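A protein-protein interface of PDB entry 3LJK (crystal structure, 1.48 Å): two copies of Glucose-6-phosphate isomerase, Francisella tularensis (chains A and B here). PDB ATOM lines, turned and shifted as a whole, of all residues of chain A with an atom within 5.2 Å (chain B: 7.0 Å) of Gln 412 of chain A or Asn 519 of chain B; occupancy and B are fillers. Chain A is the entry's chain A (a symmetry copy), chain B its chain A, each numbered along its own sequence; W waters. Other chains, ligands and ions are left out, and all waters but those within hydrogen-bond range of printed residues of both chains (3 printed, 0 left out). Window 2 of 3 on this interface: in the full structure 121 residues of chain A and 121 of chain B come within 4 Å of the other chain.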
ATOM      1  N   ASP A 408     -13.325  14.934  37.796  1.00  0.00           N
ATOM      2  CA  ASP A 408     -13.384  15.753  36.608  1.00  0.00           C
ATOM      3  C   ASP A 408     -14.304  15.145  35.550  1.00  0.00           C
ATOM      4  O   ASP A 408     -14.958  15.895  34.805  1.00  0.00           O
ATOM      5  CB  ASP A 408     -12.004  15.969  36.027  1.00  0.00           C
ATOM      6  CG  ASP A 408     -11.102  16.826  36.929  1.00  0.00           C
ATOM      7  OD1 ASP A 408     -11.586  17.503  37.839  1.00  0.00           O
ATOM      8  OD2 ASP A 408      -9.903  16.817  36.656  1.00  0.00           O
ATOM      9  N   ASN A 409     -14.397  13.802  35.504  1.00  0.00           N
ATOM     10  CA  ASN A 409     -15.301  13.159  34.552  1.00  0.00           C
ATOM     11  C   ASN A 409     -16.764  13.461  34.856  1.00  0.00           C
ATOM     12  O   ASN A 409     -17.548  13.674  33.933  1.00  0.00           O
ATOM     13  CB  ASN A 409     -15.052  11.660  34.476  1.00  0.00           C
ATOM     14  CG  ASN A 409     -15.295  10.937  35.756  1.00  0.00           C
ATOM     15  OD1 ASN A 409     -14.996  11.439  36.871  1.00  0.00           O
ATOM     16  ND2 ASN A 409     -15.886   9.732  35.618  1.00  0.00           N
ATOM     17  N   HIS A 410     -17.107  13.532  36.137  1.00  0.00           N
ATOM     18  CA  HIS A 410     -18.452  13.870  36.516  1.00  0.00           C
ATOM     19  C   HIS A 410     -18.772  15.318  36.122  1.00  0.00           C
ATOM     20  O   HIS A 410     -19.850  15.611  35.624  1.00  0.00           O
ATOM     21  CB  HIS A 410     -18.668  13.723  38.024  1.00  0.00           C
ATOM     22  CG  HIS A 410     -18.778  12.318  38.500  1.00  0.00           C
ATOM     23  ND1 HIS A 410     -19.949  11.820  39.015  1.00  0.00           N
ATOM     24  CD2 HIS A 410     -17.850  11.321  38.620  1.00  0.00           C
ATOM     25  CE1 HIS A 410     -19.742  10.565  39.410  1.00  0.00           C
ATOM     26  NE2 HIS A 410     -18.488  10.232  39.163  1.00  0.00           N
ATOM     27  N   GLN A 411     -17.855  16.237  36.401  1.00  0.00           N
ATOM     28  CA  GLN A 411     -18.084  17.657  36.088  1.00  0.00           C
ATOM     29  C   GLN A 411     -18.225  17.883  34.579  1.00  0.00           C
ATOM     30  O   GLN A 411     -19.088  18.629  34.143  1.00  0.00           O
ATOM     31  CB  GLN A 411     -16.967  18.472  36.685  1.00  0.00           C
ATOM     32  CG  GLN A 411     -17.132  19.942  36.464  1.00  0.00           C
ATOM     33  CD  GLN A 411     -18.293  20.618  37.229  1.00  0.00           C
ATOM     34  OE1 GLN A 411     -18.929  20.006  38.093  1.00  0.00           O
ATOM     35  NE2 GLN A 411     -18.545  21.901  36.917  1.00  0.00           N
ATOM     36  N   GLN A 412     -17.398  17.206  33.799  1.00  0.00           N
ATOM     37  CA  GLN A 412     -17.497  17.310  32.360  1.00  0.00           C
ATOM     38  C   GLN A 412     -18.857  16.808  31.837  1.00  0.00           C
ATOM     39  O   GLN A 412     -19.476  17.454  30.971  1.00  0.00           O
ATOM     40  CB  GLN A 412     -16.355  16.558  31.717  1.00  0.00           C
ATOM     41  CG  GLN A 412     -16.216  16.902  30.273  1.00  0.00           C
ATOM     42  CD  GLN A 412     -15.142  16.126  29.587  1.00  0.00           C
ATOM     43  OE1 GLN A 412     -15.152  14.906  29.636  1.00  0.00           O
ATOM     44  NE2 GLN A 412     -14.210  16.822  28.946  1.00  0.00           N
ATOM     45  N   ALA A 413     -19.319  15.668  32.373  1.00  0.00           N
ATOM     46  CA  ALA A 413     -20.594  15.104  31.973  1.00  0.00           C
ATOM     47  C   ALA A 413     -21.747  16.048  32.394  1.00  0.00           C
ATOM     48  O   ALA A 413     -22.718  16.208  31.665  1.00  0.00           O
ATOM     49  CB  ALA A 413     -20.795  13.751  32.583  1.00  0.00           C
ATOM     50  N   LEU A 414     -21.659  16.655  33.581  1.00  0.00           N
ATOM     51  CA  LEU A 414     -22.680  17.583  34.046  1.00  0.00           C
ATOM     52  C   LEU A 414     -22.839  18.744  33.071  1.00  0.00           C
ATOM     53  O   LEU A 414     -23.952  19.064  32.639  1.00  0.00           O
ATOM     54  CB  LEU A 414     -22.271  18.067  35.445  1.00  0.00           C
ATOM     55  CG  LEU A 414     -23.164  19.113  36.121  1.00  0.00           C
ATOM     56  CD1 LEU A 414     -24.592  18.587  36.376  1.00  0.00           C
ATOM     57  CD2 LEU A 414     -22.488  19.619  37.395  1.00  0.00           C
ATOM     58  N   LEU A 415     -21.714  19.341  32.660  1.00  0.00           N
ATOM     59  CA  LEU A 415     -21.727  20.440  31.729  1.00  0.00           C
ATOM     60  C   LEU A 415     -22.188  20.005  30.352  1.00  0.00           C
ATOM     61  O   LEU A 415     -22.958  20.719  29.685  1.00  0.00           O
ATOM     62  CB  LEU A 415     -20.367  21.105  31.665  1.00  0.00           C
ATOM     63  CG  LEU A 415     -19.961  21.854  32.930  1.00  0.00           C
ATOM     64  CD1 LEU A 415     -18.435  22.087  32.929  1.00  0.00           C
ATOM     65  CD2 LEU A 415     -20.753  23.139  33.122  1.00  0.00           C
ATOM     66  N   ALA A 416     -21.695  18.856  29.871  1.00  0.00           N
ATOM     67  CA  ALA A 416     -22.128  18.373  28.562  1.00  0.00           C
ATOM     68  C   ALA A 416     -23.644  18.196  28.498  1.00  0.00           C
ATOM     69  O   ALA A 416     -24.289  18.533  27.496  1.00  0.00           O
ATOM     70  CB  ALA A 416     -21.420  17.060  28.198  1.00  0.00           C
ATOM     71  N   ASN A 417     -24.224  17.694  29.590  1.00  0.00           N
ATOM     72  CA  ASN A 417     -25.689  17.556  29.662  1.00  0.00           C
ATOM     73  C   ASN A 417     -26.379  18.929  29.661  1.00  0.00           C
ATOM     74  O   ASN A 417     -27.392  19.113  28.988  1.00  0.00           O
ATOM     75  CB  ASN A 417     -26.095  16.775  30.913  1.00  0.00           C
ATOM     76  CG  ASN A 417     -26.055  15.266  30.695  1.00  0.00           C
ATOM     77  OD1 ASN A 417     -27.011  14.703  30.131  1.00  0.00           O
ATOM     78  ND2 ASN A 417     -24.930  14.626  31.051  1.00  0.00           N
ATOM     79  N   VAL B 178     -25.337  13.348  38.272  1.00  0.00           N
ATOM     80  CA  VAL B 178     -23.957  13.112  37.891  1.00  0.00           C
ATOM     81  C   VAL B 178     -23.010  14.120  38.550  1.00  0.00           C
ATOM     82  O   VAL B 178     -21.858  13.805  38.766  1.00  0.00           O
ATOM     83  CB  VAL B 178     -23.761  13.093  36.365  1.00  0.00           C
ATOM     84  CG1 VAL B 178     -24.038  14.441  35.710  1.00  0.00           C
ATOM     85  CG2 VAL B 178     -22.419  12.509  35.986  1.00  0.00           C
ATOM     86  N   GLU B 207     -26.583   7.259  32.028  1.00  0.00           N
ATOM     87  CA  GLU B 207     -25.259   7.853  32.133  1.00  0.00           C
ATOM     88  C   GLU B 207     -24.900   8.212  33.556  1.00  0.00           C
ATOM     89  O   GLU B 207     -23.815   7.878  34.046  1.00  0.00           O
ATOM     90  CB  GLU B 207     -25.168   9.114  31.229  1.00  0.00           C
ATOM     91  CG  GLU B 207     -23.770   9.736  31.302  1.00  0.00           C
ATOM     92  CD  GLU B 207     -23.630  11.146  30.760  1.00  0.00           C
ATOM     93  OE1 GLU B 207     -24.649  11.832  30.666  1.00  0.00           O
ATOM     94  OE2 GLU B 207     -22.468  11.553  30.404  1.00  0.00           O
ATOM     95  N   LEU B 211     -21.822   6.484  35.844  1.00  0.00           N
ATOM     96  CA  LEU B 211     -20.659   7.189  36.401  1.00  0.00           C
ATOM     97  C   LEU B 211     -20.638   7.119  37.942  1.00  0.00           C
ATOM     98  O   LEU B 211     -19.603   6.878  38.554  1.00  0.00           O
ATOM     99  CB  LEU B 211     -20.600   8.642  35.943  1.00  0.00           C
ATOM    100  CG  LEU B 211     -19.804   8.974  34.696  1.00  0.00           C
ATOM    101  CD1 LEU B 211     -20.347   8.211  33.503  1.00  0.00           C
ATOM    102  CD2 LEU B 211     -19.740  10.464  34.438  1.00  0.00           C
ATOM    103  N   ASN B 513     -22.333  13.609  21.949  1.00  0.00           N
ATOM    104  CA  ASN B 513     -21.628  14.340  20.898  1.00  0.00           C
ATOM    105  C   ASN B 513     -20.831  15.517  21.505  1.00  0.00           C
ATOM    106  O   ASN B 513     -19.686  15.775  21.157  1.00  0.00           O
ATOM    107  CB  ASN B 513     -22.632  14.953  19.918  1.00  0.00           C
ATOM    108  CG  ASN B 513     -23.361  13.961  19.039  1.00  0.00           C
ATOM    109  OD1 ASN B 513     -22.985  12.796  18.922  1.00  0.00           O
ATOM    110  ND2 ASN B 513     -24.457  14.448  18.389  1.00  0.00           N
ATOM    111  N   ILE B 514     -21.447  16.216  22.455  1.00  0.00           N
ATOM    112  CA  ILE B 514     -20.780  17.353  23.112  1.00  0.00           C
ATOM    113  C   ILE B 514     -19.595  16.895  23.984  1.00  0.00           C
ATOM    114  O   ILE B 514     -18.540  17.538  23.999  1.00  0.00           O
ATOM    115  CB  ILE B 514     -21.815  18.169  23.915  1.00  0.00           C
ATOM    116  CG1 ILE B 514     -22.748  18.926  22.939  1.00  0.00           C
ATOM    117  CG2 ILE B 514     -21.075  19.120  24.899  1.00  0.00           C
ATOM    118  CD1 ILE B 514     -24.009  19.548  23.547  1.00  0.00           C
ATOM    119  N   LEU B 515     -19.711  15.738  24.630  1.00  0.00           N
ATOM    120  CA  LEU B 515     -18.602  15.181  25.394  1.00  0.00           C
ATOM    121  C   LEU B 515     -17.421  14.929  24.472  1.00  0.00           C
ATOM    122  O   LEU B 515     -16.273  15.228  24.792  1.00  0.00           O
ATOM    123  CB  LEU B 515     -18.998  13.848  26.043  1.00  0.00           C
ATOM    124  CG  LEU B 515     -19.546  13.956  27.451  1.00  0.00           C
ATOM    125  CD1 LEU B 515     -19.989  12.597  28.001  1.00  0.00           C
ATOM    126  CD2 LEU B 515     -18.491  14.565  28.384  1.00  0.00           C
ATOM    127  N   LYS B 516     -17.694  14.362  23.297  1.00  0.00           N
ATOM    128  CA  LYS B 516     -16.630  14.130  22.294  1.00  0.00           C
ATOM    129  C   LYS B 516     -15.979  15.447  21.861  1.00  0.00           C
ATOM    130  O   LYS B 516     -14.731  15.560  21.736  1.00  0.00           O
ATOM    131  CB  LYS B 516     -17.167  13.383  21.044  1.00  0.00           C
ATOM    132  CG  LYS B 516     -17.476  11.900  21.255  1.00  0.00           C
ATOM    133  CD  LYS B 516     -18.055  11.231  19.997  1.00  0.00           C
ATOM    134  CE  LYS B 516     -18.265   9.721  20.202  1.00  0.00           C
ATOM    135  NZ  LYS B 516     -19.318   9.447  21.228  1.00  0.00           N
ATOM    136  N   ALA B 517     -16.810  16.461  21.593  1.00  0.00           N
ATOM    137  CA  ALA B 517     -16.308  17.774  21.201  1.00  0.00           C
ATOM    138  C   ALA B 517     -15.469  18.440  22.298  1.00  0.00           C
ATOM    139  O   ALA B 517     -14.503  19.098  22.031  1.00  0.00           O
ATOM    140  CB  ALA B 517     -17.463  18.673  20.812  1.00  0.00           C
ATOM    141  N   MET B 518     -15.886  18.313  23.548  1.00  0.00           N
ATOM    142  CA  MET B 518     -15.095  18.833  24.668  1.00  0.00           C
ATOM    143  C   MET B 518     -13.718  18.177  24.775  1.00  0.00           C
ATOM    144  O   MET B 518     -12.802  18.739  25.375  1.00  0.00           O
ATOM    145  CB  MET B 518     -15.850  18.615  25.978  1.00  0.00           C
ATOM    146  CG  MET B 518     -17.085  19.516  26.118  1.00  0.00           C
ATOM    147  SD  MET B 518     -18.204  19.245  27.631  1.00  0.00           S
ATOM    148  CE  MET B 518     -17.268  20.463  28.854  1.00  0.00           C
ATOM    149  N   ASN B 519     -13.584  16.980  24.240  1.00  0.00           N
ATOM    150  CA  ASN B 519     -12.307  16.250  24.377  1.00  0.00           C
ATOM    151  C   ASN B 519     -11.446  16.312  23.151  1.00  0.00           C
ATOM    152  O   ASN B 519     -10.277  15.896  23.212  1.00  0.00           O
ATOM    153  CB  ASN B 519     -12.571  14.807  24.854  1.00  0.00           C
ATOM    154  CG  ASN B 519     -12.989  14.781  26.349  1.00  0.00           C
ATOM    155  OD1 ASN B 519     -12.259  15.289  27.190  1.00  0.00           O
ATOM    156  ND2 ASN B 519     -14.177  14.273  26.659  1.00  0.00           N
ATOM    157  N   ASP B 520     -11.971  16.875  22.066  1.00  0.00           N
ATOM    158  CA  ASP B 520     -11.253  16.882  20.777  1.00  0.00           C
ATOM    159  C   ASP B 520     -11.822  17.934  19.823  1.00  0.00           C
ATOM    160  O   ASP B 520     -12.805  17.678  19.104  1.00  0.00           O
ATOM    161  CB  ASP B 520     -11.310  15.492  20.134  1.00  0.00           C
ATOM    162  CG  ASP B 520     -10.468  15.386  18.846  1.00  0.00           C
ATOM    163  OD1 ASP B 520     -10.524  14.307  18.199  1.00  0.00           O
ATOM    164  OD2 ASP B 520      -9.776  16.370  18.476  1.00  0.00           O
ATOM    165  N   ASP B 521     -11.172  19.093  19.783  1.00  0.00           N
ATOM    166  CA  ASP B 521     -11.659  20.177  18.936  1.00  0.00           C
ATOM    167  C   ASP B 521     -11.382  20.006  17.436  1.00  0.00           C
ATOM    168  O   ASP B 521     -11.788  20.867  16.649  1.00  0.00           O
ATOM    169  CB  ASP B 521     -11.248  21.570  19.476  1.00  0.00           C
ATOM    170  CG  ASP B 521      -9.738  21.829  19.450  1.00  0.00           C
ATOM    171  OD1 ASP B 521      -8.983  21.096  18.768  1.00  0.00           O
ATOM    172  OD2 ASP B 521      -9.325  22.816  20.117  1.00  0.00           O
ATOM    173  N   SER B 522     -10.743  18.892  17.051  1.00  0.00           N
ATOM    174  CA  SER B 522     -10.592  18.523  15.640  1.00  0.00           C
ATOM    175  C   SER B 522     -11.681  17.553  15.171  1.00  0.00           C
ATOM    176  O   SER B 522     -11.706  17.152  13.995  1.00  0.00           O
ATOM    177  CB  SER B 522      -9.206  17.888  15.376  1.00  0.00           C
ATOM    178  OG  SER B 522      -9.222  16.479  15.652  1.00  0.00           O
ATOM    179  N   SER B 523     -12.585  17.155  16.074  1.00  0.00           N
ATOM    180  CA  SER B 523     -13.541  16.132  15.752  1.00  0.00           C
ATOM    181  C   SER B 523     -14.633  16.701  14.863  1.00  0.00           C
ATOM    182  O   SER B 523     -14.883  17.924  14.862  1.00  0.00           O
ATOM    183  CB  SER B 523     -14.184  15.596  17.044  1.00  0.00           C
ATOM    184  OG  SER B 523     -14.789  16.654  17.796  1.00  0.00           O
ATOM    185  N   TYR B 526     -17.124  18.570  17.110  1.00  0.00           N
ATOM    186  CA  TYR B 526     -16.826  19.960  17.417  1.00  0.00           C
ATOM    187  C   TYR B 526     -17.127  20.868  16.220  1.00  0.00           C
ATOM    188  O   TYR B 526     -17.690  21.951  16.372  1.00  0.00           O
ATOM    189  CB  TYR B 526     -15.374  20.091  17.841  1.00  0.00           C
ATOM    190  CG  TYR B 526     -14.989  21.459  18.277  1.00  0.00           C
ATOM    191  CD1 TYR B 526     -14.953  21.789  19.633  1.00  0.00           C
ATOM    192  CD2 TYR B 526     -14.661  22.438  17.338  1.00  0.00           C
ATOM    193  CE1 TYR B 526     -14.611  23.060  20.043  1.00  0.00           C
ATOM    194  CE2 TYR B 526     -14.308  23.683  17.721  1.00  0.00           C
ATOM    195  CZ  TYR B 526     -14.265  23.997  19.080  1.00  0.00           C
ATOM    196  OH  TYR B 526     -13.934  25.256  19.488  1.00  0.00           O
ATOM    197  N   ILE B 537     -18.403  25.722  25.558  1.00  0.00           N
ATOM    198  CA  ILE B 537     -17.310  24.762  25.796  1.00  0.00           C
ATOM    199  C   ILE B 537     -15.992  25.513  25.939  1.00  0.00           C
ATOM    200  O   ILE B 537     -15.214  25.197  26.789  1.00  0.00           O
ATOM    201  CB  ILE B 537     -17.265  23.732  24.666  1.00  0.00           C
ATOM    202  CG1 ILE B 537     -18.473  22.807  24.758  1.00  0.00           C
ATOM    203  CG2 ILE B 537     -15.906  22.974  24.642  1.00  0.00           C
ATOM    204  CD1 ILE B 537     -18.585  21.969  23.449  1.00  0.00           C
ATOM    205  N   VAL B 540     -15.594  27.210  29.300  1.00  0.00           N
ATOM    206  CA  VAL B 540     -15.328  26.255  30.360  1.00  0.00           C
ATOM    207  C   VAL B 540     -13.849  25.935  30.393  1.00  0.00           C
ATOM    208  O   VAL B 540     -13.260  26.040  31.465  1.00  0.00           O
ATOM    209  CB  VAL B 540     -16.241  25.015  30.268  1.00  0.00           C
ATOM    210  CG1 VAL B 540     -15.752  23.919  31.145  1.00  0.00           C
ATOM    211  CG2 VAL B 540     -17.702  25.429  30.623  1.00  0.00           C
ATOM    212  N   LYS B 541     -13.273  25.665  29.215  1.00  0.00           N
ATOM    213  CA  LYS B 541     -11.866  25.246  29.094  1.00  0.00           C
ATOM    214  C   LYS B 541     -10.882  26.325  29.428  1.00  0.00           C
ATOM    215  O   LYS B 541      -9.802  26.018  29.934  1.00  0.00           O
ATOM    216  CB  LYS B 541     -11.547  24.771  27.687  1.00  0.00           C
ATOM    217  CG  LYS B 541     -12.133  23.454  27.385  1.00  0.00           C
ATOM    218  CD  LYS B 541     -11.196  22.533  26.641  1.00  0.00           C
ATOM    219  CE  LYS B 541     -11.891  21.218  26.423  1.00  0.00           C
ATOM    220  NZ  LYS B 541     -13.024  21.402  25.488  1.00  0.00           N
HETATM  221  O   HOH W   1     -17.095   7.183  36.872  1.00  0.00           O
HETATM  222  O   HOH W   2     -14.805  12.033  28.014  1.00  0.00           O
HETATM  223  O   HOH W   3     -27.180  12.065  29.460  1.00  0.00           O
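The side-chain amide oxygen of Asn 519 of chain B sits at hydrogen-bond distance from the side-chain amide nitrogen of Gln 412 of chain A. The backbone carbonyl oxygen of Val 178 of chain B lies within hydrogen-bond range of a ring nitrogen (ND1) of His 410 of chain A. The side-chain carboxylate (OE1) of Glu 207 of chain B is in hydrogen-bond range of the side-chain amide nitrogen (ND2) of Asn 417 of chain A (2.8 Å).
The side-chain amino group of Lys 541 of chain B sits at hydrogen-bond distance from the backbone carbonyl oxygen of Met 518 of chain B, at 2.7 Å. The side-chain amide nitrogen (ND2) of Asn 519 of chain B lies within hydrogen-bond range of the backbone carbonyl oxygen (O) of Leu 515 of chain B, at 3.0 Å. The backbone carbonyl oxygen of Ala 413 of chain A lies within hydrogen-bond range of the side-chain amide nitrogen of Asn 417 of chain A, at 2.8 Å.
Among the printed residues, merely in contact across the chains: Asn 409 of chain A with Leu 211 of chain B (3.9 Å), His 410 of chain A with Leu 211 of chain B (3.6 Å), Gln 412 of chain A with Leu 515 of chain B (3.6 Å), Gln 412 of chain A with Met 518 of chain B (3.8 Å), Ala 413 of chain A with Val 178 of chain B (3.97 Å), Ala 413 of chain A with Glu 207 of chain B (3.5 Å), Ala 413 of chain A with Leu 211 of chain B (3.9 Å), Leu 414 of chain A with Val 178 of chain B (3.8 Å), Leu 415 of chain A with Val 540 of chain B (3.7 Å), Ala 416 of chain A with Ile 514 of chain B (3.9 Å), Ala 416 of chain A with Leu 515 of chain B (3.7 Å) and Ala 416 of chain A with Met 518 of chain B (3.9 Å).
Of the printed residues of chain A, Leu 211 of chain B touches Asn 409, His 410 and Ala 413. Of the printed residues of chain A, Ile 514 of chain B touches Ala 416. Of the printed residues of chain A, Leu 515 of chain B touches Gln 412 and Ala 416. Lys 516 of chain B touches none of the printed residues of chain A. Of the printed residues of chain A, Met 518 of chain B touches Gln 412 (3.8 Å) and Ala 416 (3.9 Å). Asn 519 of chain B touches just one residue of chain A: Gln 412. Printed residues of chain A within 4 Å of Val 540 of chain B: Leu 415. Lys 541 of chain B touches none of the printed residues of chain A. The nearest printed residue of chain B that does not touch Gln 412 of chain A is Lys 541 of chain B (5.6 Å). The nearest printed residue of chain A that does not touch Asn 519 of chain B is Ala 413 of chain A (7.8 Å).
Hydrophobic or aromatic side chains of chain A within 4 Å of the printed part of chain B: His 410, Ala 413, Leu 415 and Ala 416. Of the 18 printed residues of chain B, 8 touch a printed residue of chain A. Among the printed residues, 15 pairs touch across the chains. Among the printed residues, no Asp or Glu carboxylate lies within 4 Å of a Lys or Arg side-chain nitrogen of the other chain.
No position is printed for both chains. Of the 15 pairs that touch across the chains among the printed residues, none has its exchanged pair printed and touching as well.
Water W2 bridges the side-chain amide nitrogen of Asn 519 of chain B (2.7 Å) and the side-chain amide oxygen of Gln 412 of chain A (3.3 Å). Water W3 bridges OD1 of Asn 417 of chain A (2.7 Å) and OE1 of Glu 207 of chain B (2.8 Å). Water W1 bridges O of Leu 211 of chain B and ND2 of Asn 409 of chain A.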
